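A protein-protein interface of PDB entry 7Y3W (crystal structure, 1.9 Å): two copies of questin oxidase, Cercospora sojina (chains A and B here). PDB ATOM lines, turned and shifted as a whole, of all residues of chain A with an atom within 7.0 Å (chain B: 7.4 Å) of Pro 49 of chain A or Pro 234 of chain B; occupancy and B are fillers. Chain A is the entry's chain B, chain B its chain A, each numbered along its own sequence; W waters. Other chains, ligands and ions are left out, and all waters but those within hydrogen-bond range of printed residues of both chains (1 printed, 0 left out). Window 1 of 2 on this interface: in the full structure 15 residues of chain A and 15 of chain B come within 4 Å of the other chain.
OE1 of Gln 232 of chain B sits at hydrogen-bond distance from N of Lys 229 of chain B (2.9 Å). N of Trp 47 of chain A lies within hydrogen-bond range of O of Gly 52 of chain A, at 2.8 Å. The backbone carbonyl oxygen of Asp 50 of chain A sits at hydrogen-bond distance from the guanidinium group of Arg 48 of chain A (3.1 Å). O of Ala 51 of chain A is in hydrogen-bond range of NH2 of Arg 48 of chain A (3.0 Å).
Water W1 bridges OG1 of Thr 231 of chain B (2.8 Å) and O of Phe 46 of chain A (2.9 Å).
Among the printed residues, pairs that only touch across the chains: Phe 46 of chain A with Thr 231 of chain B, Trp 47 of chain A with Thr 231 of chain B, Arg 48 of chain A with Thr 231 of chain B, Pro 49 of chain A with Thr 231 of chain B, Pro 49 of chain A with Gln 232 of chain B, Pro 49 of chain A with Pro 234 of chain B and Asp 50 of chain A with Asp 50 of chain B.
Of the printed residues of chain B, Arg 48 of chain A touches Thr 231 (3.7 Å). Pro 49 of chain A touches just these residues of chain B: Thr 231, Gln 232 and Pro 234. Leu 111 of chain A touches none of the printed residues of chain B. Of the printed residues of chain A, Gln 232 of chain B touches Pro 49 (3.4 Å). Printed residues of chain A within 4 Å of Pro 234 of chain B: Pro 49 (3.9 Å). The nearest printed residue of chain A that does not touch Gln 232 of chain B is Arg 48 of chain A (5.9 Å).
Asp 50 of chain B touches its own counterpart, Asp 50 of chain A. 4 positions are printed for both chains. Of the 7 pairs that touch across the chains among the printed residues, 1 has its exchanged pair printed and touching as well.
Of the 10 printed residues of chain A, 5 touch a printed residue of chain B. Printed residues of chain A that touch a printed residue of chain B: Phe 46, Trp 47, Arg 48, Pro 49 and Asp 50. Hydrophobic or aromatic side chains of chain A within 4 Å of the printed part of chain B: Pro 49. Of the 20 printed residues of chain B, 4 touch a printed residue of chain A. Hydrophobic or aromatic side chains of chain B that line the printed part of chain A: Pro 234. Among the printed residues, no Asp or Glu carboxylate lies within 4 Å of a Lys or Arg side-chain nitrogen of the other chain.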
ATOM      1  N   PHE A  46      -8.848 -14.814 -10.787  1.00  0.00           N
ATOM      2  CA  PHE A  46      -8.352 -13.530 -11.269  1.00  0.00           C
ATOM      3  C   PHE A  46      -9.215 -12.397 -10.729  1.00  0.00           C
ATOM      4  O   PHE A  46     -10.444 -12.427 -10.852  1.00  0.00           O
ATOM      5  CB  PHE A  46      -8.296 -13.509 -12.787  1.00  0.00           C
ATOM      6  CG  PHE A  46      -7.657 -14.720 -13.394  1.00  0.00           C
ATOM      7  CD1 PHE A  46      -6.287 -14.802 -13.475  1.00  0.00           C
ATOM      8  CD2 PHE A  46      -8.424 -15.697 -14.025  1.00  0.00           C
ATOM      9  CE1 PHE A  46      -5.687 -15.894 -14.064  1.00  0.00           C
ATOM     10  CE2 PHE A  46      -7.822 -16.762 -14.661  1.00  0.00           C
ATOM     11  CZ  PHE A  46      -6.448 -16.837 -14.694  1.00  0.00           C
ATOM     12  N   TRP A  47      -8.572 -11.405 -10.118  1.00  0.00           N
ATOM     13  CA  TRP A  47      -9.300 -10.306  -9.458  1.00  0.00           C
ATOM     14  C   TRP A  47      -9.092  -8.994 -10.228  1.00  0.00           C
ATOM     15  O   TRP A  47      -9.697  -8.032  -9.829  1.00  0.00           O
ATOM     16  CB  TRP A  47      -8.929 -10.208  -7.980  1.00  0.00           C
ATOM     17  CG  TRP A  47      -7.461 -10.123  -7.676  1.00  0.00           C
ATOM     18  CD1 TRP A  47      -6.610 -11.165  -7.456  1.00  0.00           C
ATOM     19  CD2 TRP A  47      -6.707  -8.933  -7.386  1.00  0.00           C
ATOM     20  NE1 TRP A  47      -5.358 -10.715  -7.170  1.00  0.00           N
ATOM     21  CE2 TRP A  47      -5.376  -9.348  -7.113  1.00  0.00           C
ATOM     22  CE3 TRP A  47      -7.010  -7.567  -7.353  1.00  0.00           C
ATOM     23  CZ2 TRP A  47      -4.360  -8.448  -6.796  1.00  0.00           C
ATOM     24  CZ3 TRP A  47      -5.994  -6.673  -7.074  1.00  0.00           C
ATOM     25  CH2 TRP A  47      -4.694  -7.107  -6.770  1.00  0.00           C
ATOM     26  N   ARG A  48      -8.209  -8.966 -11.234  1.00  0.00           N
ATOM     27  CA  ARG A  48      -8.062  -7.815 -12.168  1.00  0.00           C
ATOM     28  C   ARG A  48      -7.368  -8.330 -13.425  1.00  0.00           C
ATOM     29  O   ARG A  48      -6.869  -9.454 -13.475  1.00  0.00           O
ATOM     30  CB  ARG A  48      -7.325  -6.635 -11.510  1.00  0.00           C
ATOM     31  CG  ARG A  48      -5.915  -6.995 -11.056  1.00  0.00           C
ATOM     32  CD  ARG A  48      -5.051  -5.864 -10.481  1.00  0.00           C
ATOM     33  NE  ARG A  48      -3.743  -6.382 -10.063  1.00  0.00           N
ATOM     34  CZ  ARG A  48      -2.896  -5.757  -9.259  1.00  0.00           C
ATOM     35  NH1 ARG A  48      -3.173  -4.552  -8.822  1.00  0.00           N
ATOM     36  NH2 ARG A  48      -1.751  -6.311  -8.916  1.00  0.00           N
ATOM     37  N   PRO A  49      -7.434  -7.567 -14.536  1.00  0.00           N
ATOM     38  CA  PRO A  49      -7.060  -8.116 -15.838  1.00  0.00           C
ATOM     39  C   PRO A  49      -5.540  -8.349 -16.050  1.00  0.00           C
ATOM     40  O   PRO A  49      -5.202  -9.148 -16.908  1.00  0.00           O
ATOM     41  CB  PRO A  49      -7.689  -7.130 -16.845  1.00  0.00           C
ATOM     42  CG  PRO A  49      -8.062  -5.899 -16.067  1.00  0.00           C
ATOM     43  CD  PRO A  49      -8.066  -6.236 -14.597  1.00  0.00           C
ATOM     44  N   ASP A  50      -4.672  -7.673 -15.298  1.00  0.00           N
ATOM     45  CA  ASP A  50      -3.186  -7.847 -15.335  1.00  0.00           C
ATOM     46  C   ASP A  50      -2.657  -7.974 -13.895  1.00  0.00           C
ATOM     47  O   ASP A  50      -3.104  -7.212 -13.016  1.00  0.00           O
ATOM     48  CB  ASP A  50      -2.447  -6.667 -16.004  1.00  0.00           C
ATOM     49  CG  ASP A  50      -2.806  -6.340 -17.458  1.00  0.00           C
ATOM     50  OD1 ASP A  50      -2.668  -7.219 -18.338  1.00  0.00           O
ATOM     51  OD2 ASP A  50      -3.256  -5.222 -17.701  1.00  0.00           O
ATOM     52  N   ALA A  51      -1.722  -8.903 -13.658  1.00  0.00           N
ATOM     53  CA  ALA A  51      -1.102  -9.157 -12.344  1.00  0.00           C
ATOM     54  C   ALA A  51      -2.195  -9.425 -11.299  1.00  0.00           C
ATOM     55  O   ALA A  51      -2.074  -9.007 -10.121  1.00  0.00           O
ATOM     56  CB  ALA A  51      -0.240  -7.995 -11.983  1.00  0.00           C
ATOM     57  N   GLY A  52      -3.239 -10.147 -11.708  1.00  0.00           N
ATOM     58  CA  GLY A  52      -4.453 -10.291 -10.873  1.00  0.00           C
ATOM     59  C   GLY A  52      -4.669 -11.707 -10.381  1.00  0.00           C
ATOM     60  O   GLY A  52      -5.832 -12.077 -10.138  1.00  0.00           O
ATOM     61  N   LEU A 111      -9.921 -14.733 -19.452  1.00  0.00           N
ATOM     62  CA  LEU A 111      -9.916 -14.852 -17.973  1.00  0.00           C
ATOM     63  C   LEU A 111     -11.312 -15.204 -17.467  1.00  0.00           C
ATOM     64  O   LEU A 111     -11.401 -15.874 -16.446  1.00  0.00           O
ATOM     65  CB  LEU A 111      -9.451 -13.548 -17.334  1.00  0.00           C
ATOM     66  CG  LEU A 111      -8.056 -13.107 -17.744  1.00  0.00           C
ATOM     67  CD1 LEU A 111      -7.801 -11.729 -17.143  1.00  0.00           C
ATOM     68  CD2 LEU A 111      -7.054 -14.141 -17.277  1.00  0.00           C
ATOM     69  N   HIS A 185      -5.757 -18.270 -18.682  1.00  0.00           N
ATOM     70  CA  HIS A 185      -4.784 -17.162 -18.524  1.00  0.00           C
ATOM     71  C   HIS A 185      -4.679 -16.401 -19.842  1.00  0.00           C
ATOM     72  O   HIS A 185      -4.621 -17.042 -20.883  1.00  0.00           O
ATOM     73  CB  HIS A 185      -3.426 -17.668 -18.051  1.00  0.00           C
ATOM     74  CG  HIS A 185      -2.610 -16.572 -17.441  1.00  0.00           C
ATOM     75  ND1 HIS A 185      -2.127 -15.501 -18.193  1.00  0.00           N
ATOM     76  CD2 HIS A 185      -2.217 -16.371 -16.168  1.00  0.00           C
ATOM     77  CE1 HIS A 185      -1.434 -14.701 -17.395  1.00  0.00           C
ATOM     78  NE2 HIS A 185      -1.489 -15.212 -16.135  1.00  0.00           N
ATOM     79  N   ASP A 186      -4.772 -15.081 -19.798  1.00  0.00           N
ATOM     80  CA  ASP A 186      -4.651 -14.235 -21.013  1.00  0.00           C
ATOM     81  C   ASP A 186      -3.247 -14.482 -21.587  1.00  0.00           C
ATOM     82  O   ASP A 186      -2.303 -14.798 -20.816  1.00  0.00           O
ATOM     83  CB  ASP A 186      -4.922 -12.758 -20.715  1.00  0.00           C
ATOM     84  CG  ASP A 186      -3.918 -12.197 -19.710  1.00  0.00           C
ATOM     85  OD1 ASP A 186      -3.921 -12.693 -18.564  1.00  0.00           O
ATOM     86  OD2 ASP A 186      -3.081 -11.361 -20.092  1.00  0.00           O
ATOM     87  N   PRO B  49       0.139   1.412 -18.305  1.00  0.00           N
ATOM     88  CA  PRO B  49      -0.697   1.212 -19.496  1.00  0.00           C
ATOM     89  C   PRO B  49      -2.213   1.451 -19.359  1.00  0.00           C
ATOM     90  O   PRO B  49      -2.868   1.676 -20.373  1.00  0.00           O
ATOM     91  CB  PRO B  49      -0.452  -0.261 -19.848  1.00  0.00           C
ATOM     92  CG  PRO B  49       0.819  -0.613 -19.115  1.00  0.00           C
ATOM     93  CD  PRO B  49       0.780   0.172 -17.831  1.00  0.00           C
ATOM     94  N   ASP B  50      -2.741   1.350 -18.144  1.00  0.00           N
ATOM     95  CA  ASP B  50      -4.193   1.514 -17.860  1.00  0.00           C
ATOM     96  C   ASP B  50      -4.349   2.475 -16.673  1.00  0.00           C
ATOM     97  O   ASP B  50      -3.643   2.277 -15.668  1.00  0.00           O
ATOM     98  CB  ASP B  50      -4.894   0.189 -17.506  1.00  0.00           C
ATOM     99  CG  ASP B  50      -4.992  -0.832 -18.642  1.00  0.00           C
ATOM    100  OD1 ASP B  50      -5.512  -0.510 -19.742  1.00  0.00           O
ATOM    101  OD2 ASP B  50      -4.609  -1.935 -18.415  1.00  0.00           O
ATOM    102  N   ALA B  51      -5.240   3.478 -16.762  1.00  0.00           N
ATOM    103  CA  ALA B  51      -5.479   4.428 -15.636  1.00  0.00           C
ATOM    104  C   ALA B  51      -4.159   5.085 -15.179  1.00  0.00           C
ATOM    105  O   ALA B  51      -3.951   5.404 -13.986  1.00  0.00           O
ATOM    106  CB  ALA B  51      -6.180   3.679 -14.546  1.00  0.00           C
ATOM    107  N   GLY B 155     -10.507   7.419 -21.716  1.00  0.00           N
ATOM    108  CA  GLY B 155      -9.990   7.172 -20.360  1.00  0.00           C
ATOM    109  C   GLY B 155     -10.728   7.942 -19.281  1.00  0.00           C
ATOM    110  O   GLY B 155     -10.069   8.398 -18.330  1.00  0.00           O
ATOM    111  N   ASP B 186      -4.572   5.332 -25.710  1.00  0.00           N
ATOM    112  CA  ASP B 186      -4.996   3.995 -26.228  1.00  0.00           C
ATOM    113  C   ASP B 186      -6.519   4.016 -26.439  1.00  0.00           C
ATOM    114  O   ASP B 186      -7.234   4.742 -25.689  1.00  0.00           O
ATOM    115  CB  ASP B 186      -4.561   2.856 -25.295  1.00  0.00           C
ATOM    116  CG  ASP B 186      -5.151   2.957 -23.905  1.00  0.00           C
ATOM    117  OD1 ASP B 186      -4.822   3.953 -23.195  1.00  0.00           O
ATOM    118  OD2 ASP B 186      -6.014   2.110 -23.559  1.00  0.00           O
ATOM    119  N   ALA B 188     -10.441   2.694 -26.548  1.00  0.00           N
ATOM    120  CA  ALA B 188     -11.425   1.803 -25.878  1.00  0.00           C
ATOM    121  C   ALA B 188     -12.569   1.428 -26.838  1.00  0.00           C
ATOM    122  O   ALA B 188     -13.604   0.972 -26.344  1.00  0.00           O
ATOM    123  CB  ALA B 188     -11.928   2.437 -24.613  1.00  0.00           C
ATOM    124  N   LYS B 229     -18.033  -6.379 -16.669  1.00  0.00           N
ATOM    125  CA  LYS B 229     -17.798  -7.243 -15.500  1.00  0.00           C
ATOM    126  C   LYS B 229     -16.908  -6.477 -14.539  1.00  0.00           C
ATOM    127  O   LYS B 229     -15.988  -5.787 -14.966  1.00  0.00           O
ATOM    128  CB  LYS B 229     -17.109  -8.551 -15.884  1.00  0.00           C
ATOM    129  CG  LYS B 229     -17.736  -9.329 -17.027  1.00  0.00           C
ATOM    130  CD  LYS B 229     -19.221  -9.581 -16.902  1.00  0.00           C
ATOM    131  CE  LYS B 229     -19.716 -10.337 -18.127  1.00  0.00           C
ATOM    132  NZ  LYS B 229     -20.980  -9.799 -18.674  1.00  0.00           N
ATOM    133  N   MET B 230     -17.124  -6.718 -13.252  1.00  0.00           N
ATOM    134  CA  MET B 230     -16.353  -6.053 -12.228  1.00  0.00           C
ATOM    135  C   MET B 230     -14.851  -6.209 -12.458  1.00  0.00           C
ATOM    136  O   MET B 230     -14.127  -5.221 -12.347  1.00  0.00           O
ATOM    137  CB  MET B 230     -16.687  -6.602 -10.843  1.00  0.00           C
ATOM    138  CG  MET B 230     -16.317  -5.621  -9.730  1.00  0.00           C
ATOM    139  SD  MET B 230     -16.535  -6.436  -7.961  1.00  0.00           S
ATOM    140  CE  MET B 230     -15.466  -8.074  -7.968  1.00  0.00           C
ATOM    141  N   THR B 231     -14.390  -7.454 -12.667  1.00  0.00           N
ATOM    142  CA  THR B 231     -12.958  -7.739 -12.737  1.00  0.00           C
ATOM    143  C   THR B 231     -12.361  -7.359 -14.094  1.00  0.00           C
ATOM    144  O   THR B 231     -11.110  -7.537 -14.262  1.00  0.00           O
ATOM    145  CB  THR B 231     -12.617  -9.201 -12.394  1.00  0.00           C
ATOM    146  OG1 THR B 231     -13.321 -10.014 -13.319  1.00  0.00           O
ATOM    147  CG2 THR B 231     -12.990  -9.555 -10.982  1.00  0.00           C
ATOM    148  N   GLN B 232     -13.134  -6.767 -15.007  1.00  0.00           N
ATOM    149  CA  GLN B 232     -12.514  -6.118 -16.186  1.00  0.00           C
ATOM    150  C   GLN B 232     -11.802  -4.813 -15.760  1.00  0.00           C
ATOM    151  O   GLN B 232     -11.013  -4.291 -16.563  1.00  0.00           O
ATOM    152  CB  GLN B 232     -13.514  -5.897 -17.312  1.00  0.00           C
ATOM    153  CG  GLN B 232     -13.874  -7.168 -18.059  1.00  0.00           C
ATOM    154  CD  GLN B 232     -15.091  -6.933 -18.910  1.00  0.00           C
ATOM    155  OE1 GLN B 232     -15.922  -6.073 -18.609  1.00  0.00           O
ATOM    156  NE2 GLN B 232     -15.143  -7.633 -20.033  1.00  0.00           N
ATOM    157  N   GLY B 233     -12.102  -4.276 -14.583  1.00  0.00           N
ATOM    158  CA  GLY B 233     -11.416  -3.090 -14.006  1.00  0.00           C
ATOM    159  C   GLY B 233     -11.296  -1.975 -15.039  1.00  0.00           C
ATOM    160  O   GLY B 233     -12.314  -1.498 -15.562  1.00  0.00           O
ATOM    161  N   PRO B 234     -10.062  -1.575 -15.419  1.00  0.00           N
ATOM    162  CA  PRO B 234      -9.860  -0.414 -16.301  1.00  0.00           C
ATOM    163  C   PRO B 234     -10.234  -0.658 -17.772  1.00  0.00           C
ATOM    164  O   PRO B 234     -10.256   0.302 -18.519  1.00  0.00           O
ATOM    165  CB  PRO B 234      -8.360  -0.086 -16.128  1.00  0.00           C
ATOM    166  CG  PRO B 234      -7.748  -1.490 -15.870  1.00  0.00           C
ATOM    167  CD  PRO B 234      -8.790  -2.192 -15.017  1.00  0.00           C
ATOM    168  N   VAL B 235     -10.633  -1.872 -18.150  1.00  0.00           N
ATOM    169  CA  VAL B 235     -11.031  -2.184 -19.548  1.00  0.00           C
ATOM    170  C   VAL B 235     -12.509  -2.612 -19.623  1.00  0.00           C
ATOM    171  O   VAL B 235     -12.906  -3.217 -20.587  1.00  0.00           O
ATOM    172  CB  VAL B 235     -10.029  -3.182 -20.179  1.00  0.00           C
ATOM    173  CG1 VAL B 235      -8.669  -2.498 -20.365  1.00  0.00           C
ATOM    174  CG2 VAL B 235      -9.849  -4.496 -19.413  1.00  0.00           C
ATOM    175  N   ARG B 236     -13.323  -2.288 -18.625  1.00  0.00           N
ATOM    176  CA  ARG B 236     -14.796  -2.525 -18.672  1.00  0.00           C
ATOM    177  C   ARG B 236     -15.423  -1.895 -19.909  1.00  0.00           C
ATOM    178  O   ARG B 236     -16.333  -2.499 -20.472  1.00  0.00           O
ATOM    179  CB  ARG B 236     -15.461  -1.923 -17.447  1.00  0.00           C
ATOM    180  CG  ARG B 236     -15.198  -2.703 -16.179  1.00  0.00           C
ATOM    181  CD  ARG B 236     -15.655  -1.919 -14.986  1.00  0.00           C
ATOM    182  NE  ARG B 236     -15.323  -2.549 -13.725  1.00  0.00           N
ATOM    183  CZ  ARG B 236     -15.226  -1.918 -12.572  1.00  0.00           C
ATOM    184  NH1 ARG B 236     -15.464  -0.627 -12.508  1.00  0.00           N
ATOM    185  NH2 ARG B 236     -14.918  -2.568 -11.478  1.00  0.00           N
ATOM    186  N   VAL B 237     -15.011  -0.695 -20.310  1.00  0.00           N
ATOM    187  CA  VAL B 237     -15.626  -0.015 -21.493  1.00  0.00           C
ATOM    188  C   VAL B 237     -15.198  -0.756 -22.750  1.00  0.00           C
ATOM    189  O   VAL B 237     -16.082  -1.207 -23.513  1.00  0.00           O
ATOM    190  CB  VAL B 237     -15.299   1.491 -21.567  1.00  0.00           C
ATOM    191  CG1 VAL B 237     -15.758   2.099 -22.894  1.00  0.00           C
ATOM    192  CG2 VAL B 237     -15.925   2.194 -20.371  1.00  0.00           C
ATOM    193  N   ARG B 238     -13.884  -0.895 -22.956  1.00  0.00           N
ATOM    194  CA  ARG B 238     -13.381  -1.557 -24.181  1.00  0.00           C
ATOM    195  C   ARG B 238     -13.901  -2.994 -24.276  1.00  0.00           C
ATOM    196  O   ARG B 238     -14.483  -3.333 -25.299  1.00  0.00           O
ATOM    197  CB  ARG B 238     -11.850  -1.560 -24.239  1.00  0.00           C
ATOM    198  CG  ARG B 238     -11.274  -2.110 -25.534  1.00  0.00           C
ATOM    199  CD  ARG B 238      -9.780  -2.286 -25.406  1.00  0.00           C
ATOM    200  NE  ARG B 238      -9.476  -3.371 -24.477  1.00  0.00           N
ATOM    201  CZ  ARG B 238      -8.338  -3.516 -23.795  1.00  0.00           C
ATOM    202  NH1 ARG B 238      -7.348  -2.639 -23.878  1.00  0.00           N
ATOM    203  NH2 ARG B 238      -8.183  -4.561 -22.995  1.00  0.00           N
ATOM    204  N   ASP B 239     -13.696  -3.812 -23.263  1.00  0.00           N
ATOM    205  CA  ASP B 239     -13.945  -5.279 -23.385  1.00  0.00           C
ATOM    206  C   ASP B 239     -15.383  -5.603 -22.985  1.00  0.00           C
ATOM    207  O   ASP B 239     -15.851  -6.644 -23.384  1.00  0.00           O
ATOM    208  CB  ASP B 239     -12.924  -6.083 -22.581  1.00  0.00           C
ATOM    209  CG  ASP B 239     -11.523  -5.980 -23.178  1.00  0.00           C
ATOM    210  OD1 ASP B 239     -11.418  -5.509 -24.296  1.00  0.00           O
ATOM    211  OD2 ASP B 239     -10.546  -6.345 -22.498  1.00  0.00           O
ATOM    212  N   PHE B 293     -15.498   6.756 -11.290  1.00  0.00           N
ATOM    213  CA  PHE B 293     -15.782   7.039 -12.717  1.00  0.00           C
ATOM    214  C   PHE B 293     -16.839   8.137 -12.790  1.00  0.00           C
ATOM    215  O   PHE B 293     -16.696   9.046 -13.597  1.00  0.00           O
ATOM    216  CB  PHE B 293     -16.169   5.739 -13.436  1.00  0.00           C
ATOM    217  CG  PHE B 293     -15.129   4.671 -13.210  1.00  0.00           C
ATOM    218  CD1 PHE B 293     -13.960   4.677 -13.956  1.00  0.00           C
ATOM    219  CD2 PHE B 293     -15.285   3.712 -12.207  1.00  0.00           C
ATOM    220  CE1 PHE B 293     -12.965   3.738 -13.713  1.00  0.00           C
ATOM    221  CE2 PHE B 293     -14.281   2.787 -11.952  1.00  0.00           C
ATOM    222  CZ  PHE B 293     -13.126   2.793 -12.719  1.00  0.00           C
ATOM    223  N   TRP B 332     -20.113   5.229 -19.204  1.00  0.00           N
ATOM    224  CA  TRP B 332     -19.460   5.133 -17.871  1.00  0.00           C
ATOM    225  C   TRP B 332     -20.470   4.667 -16.803  1.00  0.00           C
ATOM    226  O   TRP B 332     -20.083   3.875 -15.933  1.00  0.00           O
ATOM    227  CB  TRP B 332     -18.687   6.420 -17.545  1.00  0.00           C
ATOM    228  CG  TRP B 332     -17.420   6.489 -18.346  1.00  0.00           C
ATOM    229  CD1 TRP B 332     -17.127   7.282 -19.421  1.00  0.00           C
ATOM    230  CD2 TRP B 332     -16.271   5.645 -18.162  1.00  0.00           C
ATOM    231  NE1 TRP B 332     -15.865   7.002 -19.896  1.00  0.00           N
ATOM    232  CE2 TRP B 332     -15.317   6.017 -19.131  1.00  0.00           C
ATOM    233  CE3 TRP B 332     -15.922   4.684 -17.213  1.00  0.00           C
ATOM    234  CZ2 TRP B 332     -14.091   5.371 -19.238  1.00  0.00           C
ATOM    235  CZ3 TRP B 332     -14.694   4.059 -17.306  1.00  0.00           C
ATOM    236  CH2 TRP B 332     -13.810   4.378 -18.329  1.00  0.00           C
ATOM    237  N   MET B 427     -14.876   1.821  -6.839  1.00  0.00           N
ATOM    238  CA  MET B 427     -14.488   1.575  -8.227  1.00  0.00           C
ATOM    239  C   MET B 427     -15.619   0.877  -8.992  1.00  0.00           C
ATOM    240  O   MET B 427     -15.374  -0.114  -9.657  1.00  0.00           O
ATOM    241  CB  MET B 427     -13.220   0.723  -8.273  1.00  0.00           C
ATOM    242  CG  MET B 427     -12.042   1.290  -7.498  1.00  0.00           C
ATOM    243  SD  MET B 427     -11.624   3.076  -8.320  1.00  0.00           S
ATOM    244  CE  MET B 427     -10.907   2.444 -10.021  1.00  0.00           C
HETATM  245  O   HOH W   1     -11.546 -12.122 -13.535  1.00  0.00           O
